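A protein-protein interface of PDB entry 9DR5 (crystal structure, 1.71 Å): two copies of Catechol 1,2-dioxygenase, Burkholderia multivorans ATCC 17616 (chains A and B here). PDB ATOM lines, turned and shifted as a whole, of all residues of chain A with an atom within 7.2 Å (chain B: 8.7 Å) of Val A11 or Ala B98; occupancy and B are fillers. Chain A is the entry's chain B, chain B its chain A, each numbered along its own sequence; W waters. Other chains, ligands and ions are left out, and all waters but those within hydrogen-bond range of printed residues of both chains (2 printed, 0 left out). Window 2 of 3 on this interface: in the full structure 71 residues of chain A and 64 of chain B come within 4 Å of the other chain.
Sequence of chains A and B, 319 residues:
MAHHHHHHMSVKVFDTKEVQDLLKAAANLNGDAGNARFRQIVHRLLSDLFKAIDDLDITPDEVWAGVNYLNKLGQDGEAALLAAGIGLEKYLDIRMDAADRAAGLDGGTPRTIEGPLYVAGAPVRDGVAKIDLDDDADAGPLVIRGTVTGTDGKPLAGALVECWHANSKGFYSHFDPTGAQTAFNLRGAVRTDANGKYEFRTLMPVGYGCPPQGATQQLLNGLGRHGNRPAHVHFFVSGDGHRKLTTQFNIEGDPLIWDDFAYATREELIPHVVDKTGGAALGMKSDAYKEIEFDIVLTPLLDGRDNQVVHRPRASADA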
ATOM      1  N   SER A  10     -35.413  -0.102  20.180  1.00  0.00           N
ATOM      2  CA  SER A  10     -33.978  -0.092  20.443  1.00  0.00           C
ATOM      3  C   SER A  10     -33.207   0.436  19.236  1.00  0.00           C
ATOM      4  O   SER A  10     -33.384  -0.047  18.116  1.00  0.00           O
ATOM      5  CB  SER A  10     -33.488  -1.497  20.802  1.00  0.00           C
ATOM      6  OG  SER A  10     -32.079  -1.521  20.991  1.00  0.00           O
ATOM      7  N   VAL A  11     -32.341   1.421  19.467  1.00  0.00           N
ATOM      8  CA  VAL A  11     -31.588   2.011  18.371  1.00  0.00           C
ATOM      9  C   VAL A  11     -30.468   1.068  17.944  1.00  0.00           C
ATOM     10  O   VAL A  11     -30.034   0.186  18.689  1.00  0.00           O
ATOM     11  CB  VAL A  11     -31.032   3.396  18.747  1.00  0.00           C
ATOM     12  CG1 VAL A  11     -32.170   4.340  19.130  1.00  0.00           C
ATOM     13  CG2 VAL A  11     -29.996   3.274  19.860  1.00  0.00           C
ATOM     14  N   LYS A  12     -30.014   1.252  16.711  1.00  0.00           N
ATOM     15  CA  LYS A  12     -28.872   0.528  16.171  1.00  0.00           C
ATOM     16  C   LYS A  12     -27.938   1.563  15.572  1.00  0.00           C
ATOM     17  O   LYS A  12     -28.247   2.159  14.532  1.00  0.00           O
ATOM     18  CB  LYS A  12     -29.294  -0.499  15.116  1.00  0.00           C
ATOM     19  CG  LYS A  12     -30.187  -1.604  15.654  1.00  0.00           C
ATOM     20  CD  LYS A  12     -29.398  -2.614  16.473  1.00  0.00           C
ATOM     21  CE  LYS A  12     -30.186  -3.060  17.701  1.00  0.00           C
ATOM     22  NZ  LYS A  12     -31.486  -3.689  17.329  1.00  0.00           N
ATOM     23  N   VAL A  13     -26.802   1.772  16.229  1.00  0.00           N
ATOM     24  CA  VAL A  13     -25.837   2.776  15.803  1.00  0.00           C
ATOM     25  C   VAL A  13     -24.500   2.186  15.398  1.00  0.00           C
ATOM     26  O   VAL A  13     -23.634   2.936  14.924  1.00  0.00           O
ATOM     27  CB  VAL A  13     -25.617   3.833  16.906  1.00  0.00           C
ATOM     28  CG1 VAL A  13     -26.946   4.474  17.293  1.00  0.00           C
ATOM     29  CG2 VAL A  13     -24.928   3.215  18.117  1.00  0.00           C
ATOM     30  N   PHE A  14     -24.286   0.882  15.577  1.00  0.00           N
ATOM     31  CA  PHE A  14     -22.936   0.343  15.443  1.00  0.00           C
ATOM     32  C   PHE A  14     -22.350   0.606  14.061  1.00  0.00           C
ATOM     33  O   PHE A  14     -21.149   0.882  13.929  1.00  0.00           O
ATOM     34  CB  PHE A  14     -22.928  -1.159  15.710  1.00  0.00           C
ATOM     35  CG  PHE A  14     -21.584  -1.779  15.493  1.00  0.00           C
ATOM     36  CD1 PHE A  14     -20.583  -1.617  16.433  1.00  0.00           C
ATOM     37  CD2 PHE A  14     -21.308  -2.498  14.353  1.00  0.00           C
ATOM     38  CE1 PHE A  14     -19.338  -2.158  16.236  1.00  0.00           C
ATOM     39  CE2 PHE A  14     -20.055  -3.054  14.155  1.00  0.00           C
ATOM     40  CZ  PHE A  14     -19.077  -2.882  15.095  1.00  0.00           C
ATOM     41  N   ILE A  53     -23.142  -4.446  22.704  1.00  0.00           N
ATOM     42  CA  ILE A  53     -23.977  -3.498  23.430  1.00  0.00           C
ATOM     43  C   ILE A  53     -25.146  -3.060  22.557  1.00  0.00           C
ATOM     44  O   ILE A  53     -26.288  -2.969  23.021  1.00  0.00           O
ATOM     45  CB  ILE A  53     -23.124  -2.298  23.887  1.00  0.00           C
ATOM     46  CG1 ILE A  53     -22.222  -2.697  25.057  1.00  0.00           C
ATOM     47  CG2 ILE A  53     -24.030  -1.111  24.243  1.00  0.00           C
ATOM     48  CD1 ILE A  53     -21.076  -1.719  25.315  1.00  0.00           C
ATOM     49  N   ASP A  54     -24.869  -2.793  21.279  1.00  0.00           N
ATOM     50  CA  ASP A  54     -25.892  -2.393  20.316  1.00  0.00           C
ATOM     51  C   ASP A  54     -26.914  -3.504  20.117  1.00  0.00           C
ATOM     52  O   ASP A  54     -28.130  -3.267  20.133  1.00  0.00           O
ATOM     53  CB  ASP A  54     -25.201  -2.041  18.990  1.00  0.00           C
ATOM     54  CG  ASP A  54     -25.972  -1.042  18.141  1.00  0.00           C
ATOM     55  OD1 ASP A  54     -26.484  -0.050  18.686  1.00  0.00           O
ATOM     56  OD2 ASP A  54     -25.996  -1.229  16.905  1.00  0.00           O
ATOM     57  N   ASP A  55     -26.430  -4.734  19.969  1.00  0.00           N
ATOM     58  CA  ASP A  55     -27.287  -5.861  19.600  1.00  0.00           C
ATOM     59  C   ASP A  55     -28.217  -6.262  20.735  1.00  0.00           C
ATOM     60  O   ASP A  55     -29.383  -6.615  20.505  1.00  0.00           O
ATOM     61  CB  ASP A  55     -26.423  -7.062  19.219  1.00  0.00           C
ATOM     62  CG  ASP A  55     -25.954  -7.039  17.777  1.00  0.00           C
ATOM     63  OD1 ASP A  55     -26.397  -6.159  17.014  1.00  0.00           O
ATOM     64  OD2 ASP A  55     -25.161  -7.940  17.402  1.00  0.00           O
ATOM     65  N   ASP A  57     -28.844  -4.257  23.311  1.00  0.00           N
ATOM     66  CA  ASP A  57     -29.310  -3.023  23.945  1.00  0.00           C
ATOM     67  C   ASP A  57     -28.887  -2.979  25.413  1.00  0.00           C
ATOM     68  O   ASP A  57     -29.698  -2.787  26.320  1.00  0.00           O
ATOM     69  CB  ASP A  57     -30.824  -2.883  23.796  1.00  0.00           C
ATOM     70  CG  ASP A  57     -31.319  -1.463  24.074  1.00  0.00           C
ATOM     71  OD1 ASP A  57     -30.514  -0.504  24.036  1.00  0.00           O
ATOM     72  OD2 ASP A  57     -32.526  -1.308  24.333  1.00  0.00           O
ATOM     73  N   TYR B  91     -19.492   6.235  23.625  1.00  0.00           N
ATOM     74  CA  TYR B  91     -20.398   5.377  22.867  1.00  0.00           C
ATOM     75  C   TYR B  91     -21.769   5.302  23.527  1.00  0.00           C
ATOM     76  O   TYR B  91     -22.803   5.307  22.838  1.00  0.00           O
ATOM     77  CB  TYR B  91     -19.761   3.998  22.730  1.00  0.00           C
ATOM     78  CG  TYR B  91     -20.564   3.007  21.926  1.00  0.00           C
ATOM     79  CD1 TYR B  91     -20.871   3.262  20.607  1.00  0.00           C
ATOM     80  CD2 TYR B  91     -20.999   1.823  22.485  1.00  0.00           C
ATOM     81  CE1 TYR B  91     -21.592   2.358  19.845  1.00  0.00           C
ATOM     82  CE2 TYR B  91     -21.715   0.900  21.722  1.00  0.00           C
ATOM     83  CZ  TYR B  91     -22.002   1.184  20.406  1.00  0.00           C
ATOM     84  OH  TYR B  91     -22.701   0.288  19.621  1.00  0.00           O
ATOM     85  N   LEU B  92     -21.806   5.235  24.864  1.00  0.00           N
ATOM     86  CA  LEU B  92     -23.093   5.240  25.552  1.00  0.00           C
ATOM     87  C   LEU B  92     -23.863   6.524  25.243  1.00  0.00           C
ATOM     88  O   LEU B  92     -25.087   6.496  25.061  1.00  0.00           O
ATOM     89  CB  LEU B  92     -22.886   5.087  27.054  1.00  0.00           C
ATOM     90  CG  LEU B  92     -22.186   3.812  27.537  1.00  0.00           C
ATOM     91  CD1 LEU B  92     -22.062   3.823  29.036  1.00  0.00           C
ATOM     92  CD2 LEU B  92     -22.940   2.566  27.057  1.00  0.00           C
ATOM     93  N   ASP B  93     -23.164   7.668  25.199  1.00  0.00           N
ATOM     94  CA  ASP B  93     -23.823   8.922  24.812  1.00  0.00           C
ATOM     95  C   ASP B  93     -24.329   8.886  23.374  1.00  0.00           C
ATOM     96  O   ASP B  93     -25.393   9.453  23.063  1.00  0.00           O
ATOM     97  CB  ASP B  93     -22.875  10.112  24.959  1.00  0.00           C
ATOM     98  CG  ASP B  93     -22.714  10.574  26.404  1.00  0.00           C
ATOM     99  OD1 ASP B  93     -23.361  10.035  27.333  1.00  0.00           O
ATOM    100  OD2 ASP B  93     -21.917  11.503  26.607  1.00  0.00           O
ATOM    101  N   ILE B  94     -23.563   8.269  22.468  1.00  0.00           N
ATOM    102  CA  ILE B  94     -24.015   8.160  21.084  1.00  0.00           C
ATOM    103  C   ILE B  94     -25.333   7.397  21.025  1.00  0.00           C
ATOM    104  O   ILE B  94     -26.241   7.760  20.275  1.00  0.00           O
ATOM    105  CB  ILE B  94     -22.934   7.495  20.209  1.00  0.00           C
ATOM    106  CG1 ILE B  94     -21.690   8.386  20.085  1.00  0.00           C
ATOM    107  CG2 ILE B  94     -23.505   7.111  18.809  1.00  0.00           C
ATOM    108  CD1 ILE B  94     -20.527   7.729  19.353  1.00  0.00           C
ATOM    109  N   ARG B  95     -25.461   6.326  21.814  1.00  0.00           N
ATOM    110  CA  ARG B  95     -26.696   5.544  21.784  1.00  0.00           C
ATOM    111  C   ARG B  95     -27.848   6.300  22.429  1.00  0.00           C
ATOM    112  O   ARG B  95     -28.983   6.234  21.948  1.00  0.00           O
ATOM    113  CB  ARG B  95     -26.501   4.185  22.466  1.00  0.00           C
ATOM    114  CG  ARG B  95     -25.483   3.313  21.755  1.00  0.00           C
ATOM    115  CD  ARG B  95     -25.510   1.831  22.167  1.00  0.00           C
ATOM    116  NE  ARG B  95     -26.584   1.122  21.473  1.00  0.00           N
ATOM    117  CZ  ARG B  95     -27.702   0.691  22.043  1.00  0.00           C
ATOM    118  NH1 ARG B  95     -27.889   0.760  23.353  1.00  0.00           N
ATOM    119  NH2 ARG B  95     -28.658   0.166  21.275  1.00  0.00           N
ATOM    120  N   MET B  96     -27.583   7.043  23.502  1.00  0.00           N
ATOM    121  CA  MET B  96     -28.640   7.888  24.055  1.00  0.00           C
ATOM    122  C   MET B  96     -29.018   9.005  23.088  1.00  0.00           C
ATOM    123  O   MET B  96     -30.199   9.361  22.969  1.00  0.00           O
ATOM    124  CB  MET B  96     -28.215   8.453  25.405  1.00  0.00           C
ATOM    125  CG  MET B  96     -28.169   7.415  26.522  1.00  0.00           C
ATOM    126  SD  MET B  96     -27.749   8.124  28.145  1.00  0.00           S
ATOM    127  CE  MET B  96     -25.958   7.992  28.149  1.00  0.00           C
ATOM    128  N   ASP B  97     -28.038   9.586  22.399  1.00  0.00           N
ATOM    129  CA  ASP B  97     -28.363  10.633  21.430  1.00  0.00           C
ATOM    130  C   ASP B  97     -29.258  10.088  20.324  1.00  0.00           C
ATOM    131  O   ASP B  97     -30.212  10.747  19.906  1.00  0.00           O
ATOM    132  CB  ASP B  97     -27.091  11.236  20.831  1.00  0.00           C
ATOM    133  CG  ASP B  97     -26.442  12.287  21.728  1.00  0.00           C
ATOM    134  OD1 ASP B  97     -27.026  12.686  22.766  1.00  0.00           O
ATOM    135  OD2 ASP B  97     -25.334  12.729  21.373  1.00  0.00           O
ATOM    136  N   ALA B  98     -28.981   8.870  19.852  1.00  0.00           N
ATOM    137  CA  ALA B  98     -29.790   8.303  18.785  1.00  0.00           C
ATOM    138  C   ALA B  98     -31.218   8.056  19.250  1.00  0.00           C
ATOM    139  O   ALA B  98     -32.171   8.268  18.491  1.00  0.00           O
ATOM    140  CB  ALA B  98     -29.145   7.010  18.285  1.00  0.00           C
ATOM    141  N   ALA B  99     -31.388   7.620  20.497  1.00  0.00           N
ATOM    142  CA  ALA B  99     -32.736   7.412  21.014  1.00  0.00           C
ATOM    143  C   ALA B  99     -33.477   8.737  21.153  1.00  0.00           C
ATOM    144  O   ALA B  99     -34.676   8.819  20.852  1.00  0.00           O
ATOM    145  CB  ALA B  99     -32.674   6.662  22.349  1.00  0.00           C
ATOM    146  N   ASP B 100     -32.772   9.799  21.562  1.00  0.00           N
ATOM    147  CA  ASP B 100     -33.410  11.111  21.666  1.00  0.00           C
ATOM    148  C   ASP B 100     -33.858  11.633  20.309  1.00  0.00           C
ATOM    149  O   ASP B 100     -34.930  12.238  20.196  1.00  0.00           O
ATOM    150  CB  ASP B 100     -32.462  12.119  22.305  1.00  0.00           C
ATOM    151  CG  ASP B 100     -32.371  11.961  23.810  1.00  0.00           C
ATOM    152  OD1 ASP B 100     -33.124  11.149  24.377  1.00  0.00           O
ATOM    153  OD2 ASP B 100     -31.560  12.675  24.426  1.00  0.00           O
ATOM    154  N   ARG B 101     -33.030  11.464  19.277  1.00  0.00           N
ATOM    155  CA  ARG B 101     -33.423  11.930  17.950  1.00  0.00           C
ATOM    156  C   ARG B 101     -34.677  11.212  17.481  1.00  0.00           C
ATOM    157  O   ARG B 101     -35.579  11.835  16.912  1.00  0.00           O
ATOM    158  CB  ARG B 101     -32.296  11.720  16.942  1.00  0.00           C
ATOM    159  CG  ARG B 101     -31.156  12.707  17.054  1.00  0.00           C
ATOM    160  CD  ARG B 101     -30.228  12.598  15.847  1.00  0.00           C
ATOM    161  NE  ARG B 101     -29.661  11.262  15.700  1.00  0.00           N
ATOM    162  CZ  ARG B 101     -28.533  10.850  16.269  1.00  0.00           C
ATOM    163  NH1 ARG B 101     -27.819  11.643  17.048  1.00  0.00           N
ATOM    164  NH2 ARG B 101     -28.108   9.612  16.039  1.00  0.00           N
ATOM    165  N   ALA B 102     -34.755   9.903  17.724  1.00  0.00           N
ATOM    166  CA  ALA B 102     -35.920   9.139  17.305  1.00  0.00           C
ATOM    167  C   ALA B 102     -37.195   9.572  18.019  1.00  0.00           C
ATOM    168  O   ALA B 102     -38.290   9.215  17.571  1.00  0.00           O
ATOM    169  CB  ALA B 102     -35.674   7.654  17.544  1.00  0.00           C
ATOM    170  N   ALA B 103     -37.085  10.316  19.119  1.00  0.00           N
ATOM    171  CA  ALA B 103     -38.248  10.713  19.905  1.00  0.00           C
ATOM    172  C   ALA B 103     -38.403  12.226  20.023  1.00  0.00           C
ATOM    173  O   ALA B 103     -39.226  12.687  20.822  1.00  0.00           O
ATOM    174  CB  ALA B 103     -38.169  10.094  21.303  1.00  0.00           C
ATOM    175  N   GLY B 104     -37.624  13.008  19.275  1.00  0.00           N
ATOM    176  CA  GLY B 104     -37.778  14.451  19.272  1.00  0.00           C
ATOM    177  C   GLY B 104     -37.233  15.169  20.487  1.00  0.00           C
ATOM    178  O   GLY B 104     -37.567  16.340  20.702  1.00  0.00           O
ATOM    179  N   LEU B 105     -36.404  14.510  21.293  1.00  0.00           N
ATOM    180  CA  LEU B 105     -35.859  15.090  22.520  1.00  0.00           C
ATOM    181  C   LEU B 105     -34.397  15.499  22.361  1.00  0.00           C
ATOM    182  O   LEU B 105     -33.599  15.367  23.298  1.00  0.00           O
ATOM    183  CB  LEU B 105     -36.011  14.100  23.669  1.00  0.00           C
ATOM    184  CG  LEU B 105     -37.440  13.764  24.089  1.00  0.00           C
ATOM    185  CD1 LEU B 105     -37.429  12.651  25.131  1.00  0.00           C
ATOM    186  CD2 LEU B 105     -38.149  15.000  24.628  1.00  0.00           C
ATOM    187  N   ASP B 106     -34.023  16.006  21.183  1.00  0.00           N
ATOM    188  CA  ASP B 106     -32.638  16.330  20.859  1.00  0.00           C
ATOM    189  C   ASP B 106     -32.391  17.834  20.728  1.00  0.00           C
ATOM    190  O   ASP B 106     -31.375  18.241  20.156  1.00  0.00           O
ATOM    191  CB  ASP B 106     -32.228  15.623  19.567  1.00  0.00           C
ATOM    192  CG  ASP B 106     -33.210  15.878  18.421  1.00  0.00           C
ATOM    193  OD1 ASP B 106     -34.430  15.994  18.684  1.00  0.00           O
ATOM    194  OD2 ASP B 106     -32.759  15.959  17.258  1.00  0.00           O
ATOM    195  N   ARG B 111     -25.731  16.418  25.797  1.00  0.00           N
ATOM    196  CA  ARG B 111     -25.062  15.647  26.828  1.00  0.00           C
ATOM    197  C   ARG B 111     -23.592  15.437  26.474  1.00  0.00           C
ATOM    198  O   ARG B 111     -23.194  15.448  25.307  1.00  0.00           O
ATOM    199  CB  ARG B 111     -25.723  14.272  27.000  1.00  0.00           C
ATOM    200  CG  ARG B 111     -25.588  13.381  25.768  1.00  0.00           C
ATOM    201  CD  ARG B 111     -26.092  11.960  26.042  1.00  0.00           C
ATOM    202  NE  ARG B 111     -27.385  11.922  26.712  1.00  0.00           N
ATOM    203  CZ  ARG B 111     -28.567  11.955  26.111  1.00  0.00           C
ATOM    204  NH1 ARG B 111     -28.681  12.116  24.808  1.00  0.00           N
ATOM    205  NH2 ARG B 111     -29.670  11.812  26.844  1.00  0.00           N
ATOM    206  N   ARG B 266     -17.874  18.743  22.357  1.00  0.00           N
ATOM    207  CA  ARG B 266     -18.982  19.024  21.454  1.00  0.00           C
ATOM    208  C   ARG B 266     -18.939  20.498  21.115  1.00  0.00           C
ATOM    209  O   ARG B 266     -18.657  21.330  21.983  1.00  0.00           O
ATOM    210  CB  ARG B 266     -20.323  18.649  22.083  1.00  0.00           C
ATOM    211  CG  ARG B 266     -20.335  17.156  22.460  1.00  0.00           C
ATOM    212  CD  ARG B 266     -21.702  16.596  22.819  1.00  0.00           C
ATOM    213  NE  ARG B 266     -22.481  16.298  21.630  1.00  0.00           N
ATOM    214  CZ  ARG B 266     -23.464  15.413  21.574  1.00  0.00           C
ATOM    215  NH1 ARG B 266     -23.801  14.684  22.624  1.00  0.00           N
ATOM    216  NH2 ARG B 266     -24.122  15.249  20.430  1.00  0.00           N
HETATM  217  O   HOH W   1     -31.538   1.551  22.571  1.00  0.00           O
HETATM  218  O   HOH W   2     -29.527   1.227  26.295  1.00  0.00           O
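OD1 of Asp A54 is in salt-bridge range of NE of Arg B95 (3.0 Å). NH1 of Arg B95 is in salt-bridge range of OD1 of Asp A57, 3.0 Å away. NH2 of Arg B95 sits at hydrogen-bond distance from O of Val A11, 2.9 Å away.
The backbone NH (N) of Val A13 is in hydrogen-bond range of the side-chain carboxylate (OD1) of Asp A54, 3.1 Å away. The side-chain carboxylate of Asp A54 sits at hydrogen-bond distance from the backbone NH of Phe A14 (3.0 Å). The side-chain hydroxyl of Ser A10 sits close to the side-chain carboxylate of Asp A57 (3.4 Å).
Arg B95 touches Ser A10. Ala B98 touches Val A11 (C to CG1, 3.8 Å). CG1 of Val A11 touches N of Ala B99 (3.6 Å). CE1 of Tyr B91 touches CG2 of Val A13 (3.9 Å). Val A13 touches Arg B95 (CG2 to CG, 3.7 Å). Ala B98 touches Val A13 (CB to CG1, 3.5 Å). CG2 of Ile A53 touches CE2 of Tyr B91 (3.97 Å). Ile A53 touches Arg B95 (CG2 to CD, 3.9 Å). CB of Asp A54 touches OH of Tyr B91, at 3.5 Å.
Of chain B, only Arg B95 (2.9 Å), Ala B98 (3.8 Å) and Ala B99 (3.6 Å) come within 4 Å of Val A11. Of chain A, only Val A11 and Val A13 come within 4 Å of Ala B98. No residue of chain B comes within 4 Å of Lys A12. Of the printed residues of chain A, Ala B99 touches Val A11 (3.6 Å). Printed residues of chain B within 4 Å of Asp A57: Arg B95. Of the printed residues of chain A, Tyr B91 touches Val A13, Ile A53 and Asp A54. Arg B101 touches none of the printed residues of chain A. The nearest residue of chain B that does not touch Val A11 is Ala B102 (5.1 Å). The nearest printed residue of chain A that does not touch Tyr B91 is Phe A14 (4.2 Å).
Of the 18 printed residues of chain B, 4 touch a printed residue of chain A. Of the 9 printed residues of chain A, 6 touch a printed residue of chain B. Printed residues of chain A that touch a printed residue of chain B: Ser A10, Val A11, Val A13, Ile A53, Asp A54 and Asp A57. Hydrophobic or aromatic side chains of chain A that line the printed part of chain B: Val A11, Val A13 and Ile A53.
No position is printed for both chains. Of the 12 pairs that touch across the chains among the printed residues, none has its exchanged pair printed and touching as well.
Water W1 lies within hydrogen-bond range of OD1 of Asp A57, N of Val A11, NH2 of Arg B95 and OG of Ser A10. Water W2 bridges OD1 of Asp A57 (3.0 Å) and NH1 of Arg B95 (3.4 Å).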
